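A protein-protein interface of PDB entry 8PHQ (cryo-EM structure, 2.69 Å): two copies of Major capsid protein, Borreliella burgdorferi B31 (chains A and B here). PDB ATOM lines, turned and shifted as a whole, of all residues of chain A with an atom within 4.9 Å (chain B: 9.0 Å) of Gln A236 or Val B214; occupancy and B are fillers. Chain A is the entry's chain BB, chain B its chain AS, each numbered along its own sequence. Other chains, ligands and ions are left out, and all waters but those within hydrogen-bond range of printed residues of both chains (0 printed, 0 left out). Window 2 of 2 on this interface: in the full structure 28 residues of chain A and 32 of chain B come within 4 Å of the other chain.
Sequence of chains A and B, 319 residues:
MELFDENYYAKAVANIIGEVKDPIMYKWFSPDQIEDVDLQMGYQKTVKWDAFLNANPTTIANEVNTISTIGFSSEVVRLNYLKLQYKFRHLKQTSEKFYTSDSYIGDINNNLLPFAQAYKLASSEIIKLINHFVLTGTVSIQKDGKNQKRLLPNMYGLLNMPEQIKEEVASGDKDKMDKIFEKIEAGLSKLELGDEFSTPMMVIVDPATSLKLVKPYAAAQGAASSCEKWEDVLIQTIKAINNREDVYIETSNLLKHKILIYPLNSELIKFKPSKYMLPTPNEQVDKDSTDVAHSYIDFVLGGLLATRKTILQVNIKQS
OG of Ser B210 lies within hydrogen-bond range of NH1 of Arg A244, 2.6 Å away. The side-chain hydroxyl (OG) of Ser B210 lies within hydrogen-bond range of the backbone carbonyl oxygen (O) of Ala A240, at 3.1 Å. NZ of Lys B229 lies within salt-bridge range of OE1 of Glu A228 (3.3 Å). The guanidinium group of Arg A244 is in salt-bridge range of the side-chain carboxylate of Glu B231 (2.8 Å).
O of Leu B213 is in hydrogen-bond range of N of Glu B231, at 3.4 Å. O of Lys A239 is in hydrogen-bond range of N of Arg A244, 2.9 Å away. OE2 of Glu A228 lies close to OE1 of Gln A236 (3.1 Å).
SG of Cys B227 touches CB of Glu A228 (3.99 Å). O of Gln A236 touches CG1 of Val B214, 3.8 Å away. Lys B229 touches Gln A236. CB of Ala A240 touches CD2 of Leu B211, 3.6 Å away. Val B214 touches Ala A240. Arg A244 touches Thr B251 (NH1 to OG1, 3.5 Å).
Gln A236 touches just these residues of chain B: Val B214 and Lys B229. No residue of chain B comes within 4 Å of Thr A237. Of the printed residues of chain B, Ala A240 touches Ser B210, Leu B211 and Val B214. Thr B209 touches none of the printed residues of chain A. Leu B213 touches none of the printed residues of chain A. Val B214 touches two residues of chain A. Of the printed residues of chain A, Cys B227 touches Glu A228. Of the printed residues of chain A, Glu B231 touches Arg A244 (2.8 Å).
Of the 11 printed residues of chain A, 4 touch a printed residue of chain B. Printed residues of chain A that touch a printed residue of chain B: Glu A228, Gln A236, Ala A240 and Arg A244. Hydrophobic or aromatic side chains of chain A that line the printed part of chain B: Ala A240. Of the 21 printed residues of chain B, 7 touch a printed residue of chain A. Printed residues of chain B that touch a printed residue of chain A: Ser B210, Leu B211, Val B214, Cys B227, Lys B229, Glu B231 and Thr B251. Hydrophobic or aromatic side chains of chain B that line the printed part of chain A: Leu B211 and Val B214.
Positions printed for both chains: 228 and 232. Of the 10 pairs that touch across the chains among the printed residues, none has its exchanged pair printed and touching as well.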
ATOM      1  N   GLU A 228      15.019  -5.468  31.224  1.00  0.00           N
ATOM      2  CA  GLU A 228      14.546  -6.824  31.005  1.00  0.00           C
ATOM      3  C   GLU A 228      13.396  -7.122  31.958  1.00  0.00           C
ATOM      4  O   GLU A 228      13.327  -6.575  33.062  1.00  0.00           O
ATOM      5  CB  GLU A 228      15.676  -7.842  31.201  1.00  0.00           C
ATOM      6  CG  GLU A 228      15.328  -9.256  30.774  1.00  0.00           C
ATOM      7  CD  GLU A 228      16.473 -10.222  30.980  1.00  0.00           C
ATOM      8  OE1 GLU A 228      17.532  -9.790  31.482  1.00  0.00           O
ATOM      9  OE2 GLU A 228      16.315 -11.413  30.637  1.00  0.00           O
ATOM     10  N   ASP A 232      10.829 -12.307  30.235  1.00  0.00           N
ATOM     11  CA  ASP A 232      12.002 -12.622  29.426  1.00  0.00           C
ATOM     12  C   ASP A 232      12.963 -13.532  30.180  1.00  0.00           C
ATOM     13  O   ASP A 232      13.524 -14.469  29.598  1.00  0.00           O
ATOM     14  CB  ASP A 232      12.705 -11.336  28.999  1.00  0.00           C
ATOM     15  CG  ASP A 232      11.784 -10.383  28.266  1.00  0.00           C
ATOM     16  OD1 ASP A 232      10.603 -10.732  28.062  1.00  0.00           O
ATOM     17  OD2 ASP A 232      12.242  -9.282  27.897  1.00  0.00           O
ATOM     18  N   VAL A 233      13.165 -13.271  31.474  1.00  0.00           N
ATOM     19  CA  VAL A 233      14.049 -14.129  32.263  1.00  0.00           C
ATOM     20  C   VAL A 233      13.509 -15.553  32.311  1.00  0.00           C
ATOM     21  O   VAL A 233      14.262 -16.524  32.156  1.00  0.00           O
ATOM     22  CB  VAL A 233      14.244 -13.548  33.676  1.00  0.00           C
ATOM     23  CG1 VAL A 233      15.274 -14.359  34.438  1.00  0.00           C
ATOM     24  CG2 VAL A 233      14.683 -12.102  33.590  1.00  0.00           C
ATOM     25  N   LEU A 234      12.199 -15.702  32.519  1.00  0.00           N
ATOM     26  CA  LEU A 234      11.594 -17.030  32.557  1.00  0.00           C
ATOM     27  C   LEU A 234      11.724 -17.741  31.215  1.00  0.00           C
ATOM     28  O   LEU A 234      12.022 -18.943  31.166  1.00  0.00           O
ATOM     29  CB  LEU A 234      10.126 -16.917  32.967  1.00  0.00           C
ATOM     30  CG  LEU A 234       9.274 -18.184  32.895  1.00  0.00           C
ATOM     31  CD1 LEU A 234       9.519 -19.067  34.106  1.00  0.00           C
ATOM     32  CD2 LEU A 234       7.804 -17.825  32.775  1.00  0.00           C
ATOM     33  N   ILE A 235      11.497 -17.018  30.115  1.00  0.00           N
ATOM     34  CA  ILE A 235      11.608 -17.627  28.793  1.00  0.00           C
ATOM     35  C   ILE A 235      13.032 -18.101  28.541  1.00  0.00           C
ATOM     36  O   ILE A 235      13.249 -19.203  28.025  1.00  0.00           O
ATOM     37  CB  ILE A 235      11.132 -16.650  27.703  1.00  0.00           C
ATOM     38  CG1 ILE A 235       9.647 -16.338  27.879  1.00  0.00           C
ATOM     39  CG2 ILE A 235      11.394 -17.219  26.320  1.00  0.00           C
ATOM     40  CD1 ILE A 235       9.116 -15.315  26.902  1.00  0.00           C
ATOM     41  N   GLN A 236      14.025 -17.286  28.904  1.00  0.00           N
ATOM     42  CA  GLN A 236      15.413 -17.709  28.730  1.00  0.00           C
ATOM     43  C   GLN A 236      15.742 -18.915  29.603  1.00  0.00           C
ATOM     44  O   GLN A 236      16.451 -19.832  29.169  1.00  0.00           O
ATOM     45  CB  GLN A 236      16.361 -16.550  29.028  1.00  0.00           C
ATOM     46  CG  GLN A 236      16.221 -15.387  28.068  1.00  0.00           C
ATOM     47  CD  GLN A 236      16.854 -14.119  28.598  1.00  0.00           C
ATOM     48  OE1 GLN A 236      17.428 -14.106  29.686  1.00  0.00           O
ATOM     49  NE2 GLN A 236      16.750 -13.041  27.831  1.00  0.00           N
ATOM     50  N   THR A 237      15.236 -18.937  30.838  1.00  0.00           N
ATOM     51  CA  THR A 237      15.506 -20.067  31.720  1.00  0.00           C
ATOM     52  C   THR A 237      14.930 -21.364  31.159  1.00  0.00           C
ATOM     53  O   THR A 237      15.581 -22.412  31.209  1.00  0.00           O
ATOM     54  CB  THR A 237      14.950 -19.786  33.115  1.00  0.00           C
ATOM     55  OG1 THR A 237      15.474 -18.543  33.594  1.00  0.00           O
ATOM     56  CG2 THR A 237      15.351 -20.889  34.075  1.00  0.00           C
ATOM     57  N   ILE A 238      13.708 -21.314  30.625  1.00  0.00           N
ATOM     58  CA  ILE A 238      13.121 -22.516  30.034  1.00  0.00           C
ATOM     59  C   ILE A 238      13.832 -22.895  28.737  1.00  0.00           C
ATOM     60  O   ILE A 238      13.973 -24.087  28.415  1.00  0.00           O
ATOM     61  CB  ILE A 238      11.610 -22.317  29.824  1.00  0.00           C
ATOM     62  CG1 ILE A 238      10.948 -21.946  31.148  1.00  0.00           C
ATOM     63  CG2 ILE A 238      10.979 -23.573  29.252  1.00  0.00           C
ATOM     64  CD1 ILE A 238       9.487 -21.633  31.029  1.00  0.00           C
ATOM     65  N   LYS A 239      14.272 -21.900  27.963  1.00  0.00           N
ATOM     66  CA  LYS A 239      15.052 -22.178  26.766  1.00  0.00           C
ATOM     67  C   LYS A 239      16.388 -22.819  27.099  1.00  0.00           C
ATOM     68  O   LYS A 239      16.961 -23.514  26.253  1.00  0.00           O
ATOM     69  CB  LYS A 239      15.264 -20.888  25.971  1.00  0.00           C
ATOM     70  CG  LYS A 239      14.127 -20.556  25.024  1.00  0.00           C
ATOM     71  CD  LYS A 239      14.410 -19.289  24.242  1.00  0.00           C
ATOM     72  CE  LYS A 239      13.327 -19.019  23.211  1.00  0.00           C
ATOM     73  NZ  LYS A 239      13.271 -20.078  22.170  1.00  0.00           N
ATOM     74  N   ALA A 240      16.892 -22.598  28.312  1.00  0.00           N
ATOM     75  CA  ALA A 240      18.125 -23.251  28.730  1.00  0.00           C
ATOM     76  C   ALA A 240      17.969 -24.763  28.814  1.00  0.00           C
ATOM     77  O   ALA A 240      18.950 -25.493  28.638  1.00  0.00           O
ATOM     78  CB  ALA A 240      18.582 -22.703  30.080  1.00  0.00           C
ATOM     79  N   ARG A 244      16.679 -24.655  23.566  1.00  0.00           N
ATOM     80  CA  ARG A 244      16.428 -23.356  22.942  1.00  0.00           C
ATOM     81  C   ARG A 244      15.408 -23.457  21.806  1.00  0.00           C
ATOM     82  O   ARG A 244      15.657 -23.049  20.670  1.00  0.00           O
ATOM     83  CB  ARG A 244      17.732 -22.721  22.448  1.00  0.00           C
ATOM     84  CG  ARG A 244      18.653 -22.254  23.555  1.00  0.00           C
ATOM     85  CD  ARG A 244      20.071 -22.061  23.043  1.00  0.00           C
ATOM     86  NE  ARG A 244      21.006 -21.684  24.098  1.00  0.00           N
ATOM     87  CZ  ARG A 244      21.306 -22.429  25.154  1.00  0.00           C
ATOM     88  NH1 ARG A 244      20.813 -23.647  25.308  1.00  0.00           N
ATOM     89  NH2 ARG A 244      22.136 -21.944  26.074  1.00  0.00           N
ATOM     90  N   MET B 177      31.804 -18.595  35.453  1.00  0.00           N
ATOM     91  CA  MET B 177      31.594 -18.441  34.021  1.00  0.00           C
ATOM     92  C   MET B 177      32.658 -17.555  33.396  1.00  0.00           C
ATOM     93  O   MET B 177      33.016 -17.748  32.232  1.00  0.00           O
ATOM     94  CB  MET B 177      30.203 -17.868  33.749  1.00  0.00           C
ATOM     95  CG  MET B 177      29.181 -18.899  33.301  1.00  0.00           C
ATOM     96  SD  MET B 177      29.575 -19.727  31.747  1.00  0.00           S
ATOM     97  CE  MET B 177      30.108 -18.352  30.733  1.00  0.00           C
ATOM     98  N   VAL B 205      27.108 -28.007  23.856  1.00  0.00           N
ATOM     99  CA  VAL B 205      27.263 -27.820  25.293  1.00  0.00           C
ATOM    100  C   VAL B 205      26.426 -28.859  26.030  1.00  0.00           C
ATOM    101  O   VAL B 205      25.597 -29.556  25.446  1.00  0.00           O
ATOM    102  CB  VAL B 205      26.868 -26.400  25.744  1.00  0.00           C
ATOM    103  CG1 VAL B 205      27.836 -25.378  25.183  1.00  0.00           C
ATOM    104  CG2 VAL B 205      25.448 -26.086  25.318  1.00  0.00           C
ATOM    105  N   PRO B 207      23.908 -29.634  29.640  1.00  0.00           N
ATOM    106  CA  PRO B 207      22.811 -28.868  30.264  1.00  0.00           C
ATOM    107  C   PRO B 207      23.254 -27.890  31.341  1.00  0.00           C
ATOM    108  O   PRO B 207      22.723 -26.772  31.407  1.00  0.00           O
ATOM    109  CB  PRO B 207      21.921 -29.975  30.843  1.00  0.00           C
ATOM    110  CG  PRO B 207      22.146 -31.128  29.939  1.00  0.00           C
ATOM    111  CD  PRO B 207      23.608 -31.077  29.605  1.00  0.00           C
ATOM    112  N   ALA B 208      24.216 -28.270  32.185  1.00  0.00           N
ATOM    113  CA  ALA B 208      24.705 -27.341  33.199  1.00  0.00           C
ATOM    114  C   ALA B 208      25.379 -26.137  32.556  1.00  0.00           C
ATOM    115  O   ALA B 208      25.197 -24.996  33.001  1.00  0.00           O
ATOM    116  CB  ALA B 208      25.665 -28.055  34.148  1.00  0.00           C
ATOM    117  N   THR B 209      26.161 -26.371  31.501  1.00  0.00           N
ATOM    118  CA  THR B 209      26.804 -25.269  30.800  1.00  0.00           C
ATOM    119  C   THR B 209      25.772 -24.337  30.180  1.00  0.00           C
ATOM    120  O   THR B 209      25.936 -23.116  30.217  1.00  0.00           O
ATOM    121  CB  THR B 209      27.750 -25.806  29.728  1.00  0.00           C
ATOM    122  OG1 THR B 209      28.813 -26.536  30.351  1.00  0.00           O
ATOM    123  CG2 THR B 209      28.345 -24.668  28.915  1.00  0.00           C
ATOM    124  N   SER B 210      24.702 -24.893  29.607  1.00  0.00           N
ATOM    125  CA  SER B 210      23.640 -24.054  29.056  1.00  0.00           C
ATOM    126  C   SER B 210      22.969 -23.223  30.146  1.00  0.00           C
ATOM    127  O   SER B 210      22.665 -22.036  29.946  1.00  0.00           O
ATOM    128  CB  SER B 210      22.614 -24.928  28.336  1.00  0.00           C
ATOM    129  OG  SER B 210      21.568 -24.148  27.790  1.00  0.00           O
ATOM    130  N   LEU B 211      22.729 -23.837  31.307  1.00  0.00           N
ATOM    131  CA  LEU B 211      22.158 -23.106  32.432  1.00  0.00           C
ATOM    132  C   LEU B 211      23.063 -21.957  32.852  1.00  0.00           C
ATOM    133  O   LEU B 211      22.583 -20.880  33.224  1.00  0.00           O
ATOM    134  CB  LEU B 211      21.916 -24.051  33.609  1.00  0.00           C
ATOM    135  CG  LEU B 211      20.778 -25.067  33.500  1.00  0.00           C
ATOM    136  CD1 LEU B 211      20.643 -25.838  34.797  1.00  0.00           C
ATOM    137  CD2 LEU B 211      19.468 -24.385  33.158  1.00  0.00           C
ATOM    138  N   LYS B 212      24.378 -22.173  32.822  1.00  0.00           N
ATOM    139  CA  LYS B 212      25.300 -21.083  33.130  1.00  0.00           C
ATOM    140  C   LYS B 212      25.323 -20.031  32.027  1.00  0.00           C
ATOM    141  O   LYS B 212      25.477 -18.839  32.313  1.00  0.00           O
ATOM    142  CB  LYS B 212      26.704 -21.630  33.367  1.00  0.00           C
ATOM    143  CG  LYS B 212      26.789 -22.646  34.486  1.00  0.00           C
ATOM    144  CD  LYS B 212      28.206 -23.153  34.656  1.00  0.00           C
ATOM    145  CE  LYS B 212      28.303 -24.140  35.802  1.00  0.00           C
ATOM    146  NZ  LYS B 212      29.680 -24.690  35.927  1.00  0.00           N
ATOM    147  N   LEU B 213      25.178 -20.450  30.768  1.00  0.00           N
ATOM    148  CA  LEU B 213      25.234 -19.515  29.650  1.00  0.00           C
ATOM    149  C   LEU B 213      24.055 -18.557  29.653  1.00  0.00           C
ATOM    150  O   LEU B 213      24.203 -17.397  29.256  1.00  0.00           O
ATOM    151  CB  LEU B 213      25.276 -20.261  28.317  1.00  0.00           C
ATOM    152  CG  LEU B 213      26.512 -21.073  27.927  1.00  0.00           C
ATOM    153  CD1 LEU B 213      26.397 -21.516  26.480  1.00  0.00           C
ATOM    154  CD2 LEU B 213      27.781 -20.272  28.146  1.00  0.00           C
ATOM    155  N   VAL B 214      22.874 -19.018  30.074  1.00  0.00           N
ATOM    156  CA  VAL B 214      21.715 -18.122  30.055  1.00  0.00           C
ATOM    157  C   VAL B 214      21.754 -17.075  31.156  1.00  0.00           C
ATOM    158  O   VAL B 214      20.838 -16.247  31.236  1.00  0.00           O
ATOM    159  CB  VAL B 214      20.383 -18.894  30.147  1.00  0.00           C
ATOM    160  CG1 VAL B 214      20.235 -19.813  28.950  1.00  0.00           C
ATOM    161  CG2 VAL B 214      20.299 -19.665  31.451  1.00  0.00           C
ATOM    162  N   LYS B 215      22.785 -17.075  32.001  1.00  0.00           N
ATOM    163  CA  LYS B 215      22.912 -16.076  33.050  1.00  0.00           C
ATOM    164  C   LYS B 215      23.379 -14.736  32.481  1.00  0.00           C
ATOM    165  O   LYS B 215      23.961 -14.678  31.396  1.00  0.00           O
ATOM    166  CB  LYS B 215      23.885 -16.559  34.122  1.00  0.00           C
ATOM    167  CG  LYS B 215      23.479 -17.872  34.760  1.00  0.00           C
ATOM    168  CD  LYS B 215      22.039 -17.807  35.238  1.00  0.00           C
ATOM    169  CE  LYS B 215      21.546 -19.158  35.721  1.00  0.00           C
ATOM    170  NZ  LYS B 215      20.103 -19.114  36.080  1.00  0.00           N
ATOM    171  N   PRO B 216      23.119 -13.640  33.198  1.00  0.00           N
ATOM    172  CA  PRO B 216      23.618 -12.333  32.754  1.00  0.00           C
ATOM    173  C   PRO B 216      25.137 -12.286  32.734  1.00  0.00           C
ATOM    174  O   PRO B 216      25.814 -12.950  33.522  1.00  0.00           O
ATOM    175  CB  PRO B 216      23.044 -11.365  33.795  1.00  0.00           C
ATOM    176  CG  PRO B 216      21.834 -12.059  34.312  1.00  0.00           C
ATOM    177  CD  PRO B 216      22.207 -13.511  34.347  1.00  0.00           C
ATOM    178  N   TYR B 217      25.669 -11.487  31.814  1.00  0.00           N
ATOM    179  CA  TYR B 217      27.111 -11.358  31.632  1.00  0.00           C
ATOM    180  C   TYR B 217      27.664 -10.388  32.669  1.00  0.00           C
ATOM    181  O   TYR B 217      27.325  -9.200  32.664  1.00  0.00           O
ATOM    182  CB  TYR B 217      27.423 -10.885  30.216  1.00  0.00           C
ATOM    183  CG  TYR B 217      28.837 -10.392  30.023  1.00  0.00           C
ATOM    184  CD1 TYR B 217      29.921 -11.226  30.251  1.00  0.00           C
ATOM    185  CD2 TYR B 217      29.087  -9.091  29.609  1.00  0.00           C
ATOM    186  CE1 TYR B 217      31.215 -10.780  30.073  1.00  0.00           C
ATOM    187  CE2 TYR B 217      30.377  -8.636  29.429  1.00  0.00           C
ATOM    188  CZ  TYR B 217      31.437  -9.483  29.661  1.00  0.00           C
ATOM    189  OH  TYR B 217      32.724  -9.032  29.482  1.00  0.00           O
ATOM    190  N   CYS B 227      22.633  -5.818  29.800  1.00  0.00           N
ATOM    191  CA  CYS B 227      21.465  -6.664  29.590  1.00  0.00           C
ATOM    192  C   CYS B 227      21.830  -7.776  28.606  1.00  0.00           C
ATOM    193  O   CYS B 227      20.965  -8.437  28.033  1.00  0.00           O
ATOM    194  CB  CYS B 227      20.285  -5.827  29.083  1.00  0.00           C
ATOM    195  SG  CYS B 227      18.712  -6.706  28.871  1.00  0.00           S
ATOM    196  N   GLU B 228      23.130  -7.980  28.423  1.00  0.00           N
ATOM    197  CA  GLU B 228      23.649  -8.973  27.496  1.00  0.00           C
ATOM    198  C   GLU B 228      23.995 -10.256  28.243  1.00  0.00           C
ATOM    199  O   GLU B 228      24.381 -10.230  29.414  1.00  0.00           O
ATOM    200  CB  GLU B 228      24.881  -8.434  26.765  1.00  0.00           C
ATOM    201  CG  GLU B 228      25.479  -9.384  25.744  1.00  0.00           C
ATOM    202  CD  GLU B 228      26.478  -8.701  24.833  1.00  0.00           C
ATOM    203  OE1 GLU B 228      26.690  -7.482  24.991  1.00  0.00           O
ATOM    204  OE2 GLU B 228      27.047  -9.384  23.957  1.00  0.00           O
ATOM    205  N   LYS B 229      23.841 -11.384  27.558  1.00  0.00           N
ATOM    206  CA  LYS B 229      24.067 -12.693  28.148  1.00  0.00           C
ATOM    207  C   LYS B 229      25.403 -13.287  27.709  1.00  0.00           C
ATOM    208  O   LYS B 229      25.985 -12.908  26.685  1.00  0.00           O
ATOM    209  CB  LYS B 229      22.930 -13.651  27.782  1.00  0.00           C
ATOM    210  CG  LYS B 229      21.552 -13.142  28.159  1.00  0.00           C
ATOM    211  CD  LYS B 229      21.478 -12.787  29.635  1.00  0.00           C
ATOM    212  CE  LYS B 229      20.098 -12.275  30.008  1.00  0.00           C
ATOM    213  NZ  LYS B 229      19.978 -12.012  31.467  1.00  0.00           N
ATOM    214  N   TRP B 230      25.877 -14.244  28.512  1.00  0.00           N
ATOM    215  CA  TRP B 230      27.108 -14.955  28.190  1.00  0.00           C
ATOM    216  C   TRP B 230      27.005 -15.647  26.839  1.00  0.00           C
ATOM    217  O   TRP B 230      27.997 -15.737  26.108  1.00  0.00           O
ATOM    218  CB  TRP B 230      27.418 -15.986  29.274  1.00  0.00           C
ATOM    219  CG  TRP B 230      28.028 -15.425  30.520  1.00  0.00           C
ATOM    220  CD1 TRP B 230      27.417 -15.276  31.730  1.00  0.00           C
ATOM    221  CD2 TRP B 230      29.368 -14.946  30.687  1.00  0.00           C
ATOM    222  NE1 TRP B 230      28.290 -14.733  32.638  1.00  0.00           N
ATOM    223  CE2 TRP B 230      29.495 -14.522  32.023  1.00  0.00           C
ATOM    224  CE3 TRP B 230      30.470 -14.835  29.837  1.00  0.00           C
ATOM    225  CZ2 TRP B 230      30.678 -13.994  32.528  1.00  0.00           C
ATOM    226  CZ3 TRP B 230      31.646 -14.311  30.341  1.00  0.00           C
ATOM    227  CH2 TRP B 230      31.740 -13.897  31.674  1.00  0.00           C
ATOM    228  N   GLU B 231      25.814 -16.139  26.496  1.00  0.00           N
ATOM    229  CA  GLU B 231      25.609 -16.772  25.199  1.00  0.00           C
ATOM    230  C   GLU B 231      25.830 -15.780  24.065  1.00  0.00           C
ATOM    231  O   GLU B 231      26.491 -16.099  23.069  1.00  0.00           O
ATOM    232  CB  GLU B 231      24.201 -17.361  25.141  1.00  0.00           C
ATOM    233  CG  GLU B 231      23.877 -18.127  23.878  1.00  0.00           C
ATOM    234  CD  GLU B 231      22.506 -18.776  23.938  1.00  0.00           C
ATOM    235  OE1 GLU B 231      21.823 -18.633  24.973  1.00  0.00           O
ATOM    236  OE2 GLU B 231      22.111 -19.430  22.951  1.00  0.00           O
ATOM    237  N   ASP B 232      25.300 -14.565  24.208  1.00  0.00           N
ATOM    238  CA  ASP B 232      25.517 -13.535  23.199  1.00  0.00           C
ATOM    239  C   ASP B 232      26.991 -13.173  23.096  1.00  0.00           C
ATOM    240  O   ASP B 232      27.517 -12.982  21.991  1.00  0.00           O
ATOM    241  CB  ASP B 232      24.685 -12.295  23.524  1.00  0.00           C
ATOM    242  CG  ASP B 232      23.210 -12.605  23.664  1.00  0.00           C
ATOM    243  OD1 ASP B 232      22.823 -13.775  23.464  1.00  0.00           O
ATOM    244  OD2 ASP B 232      22.437 -11.676  23.979  1.00  0.00           O
ATOM    245  N   ILE B 249      24.196 -23.208  18.142  1.00  0.00           N
ATOM    246  CA  ILE B 249      24.397 -23.716  19.494  1.00  0.00           C
ATOM    247  C   ILE B 249      23.444 -24.879  19.715  1.00  0.00           C
ATOM    248  O   ILE B 249      22.243 -24.764  19.443  1.00  0.00           O
ATOM    249  CB  ILE B 249      24.180 -22.620  20.552  1.00  0.00           C
ATOM    250  CG1 ILE B 249      25.157 -21.468  20.324  1.00  0.00           C
ATOM    251  CG2 ILE B 249      24.349 -23.188  21.949  1.00  0.00           C
ATOM    252  CD1 ILE B 249      25.159 -20.446  21.431  1.00  0.00           C
ATOM    253  N   THR B 251      22.540 -28.402  22.434  1.00  0.00           N
ATOM    254  CA  THR B 251      22.677 -29.009  23.748  1.00  0.00           C
ATOM    255  C   THR B 251      22.512 -30.514  23.610  1.00  0.00           C
ATOM    256  O   THR B 251      21.604 -30.980  22.914  1.00  0.00           O
ATOM    257  CB  THR B 251      21.643 -28.450  24.729  1.00  0.00           C
ATOM    258  OG1 THR B 251      21.729 -27.020  24.751  1.00  0.00           O
ATOM    259  CG2 THR B 251      21.897 -28.981  26.128  1.00  0.00           C
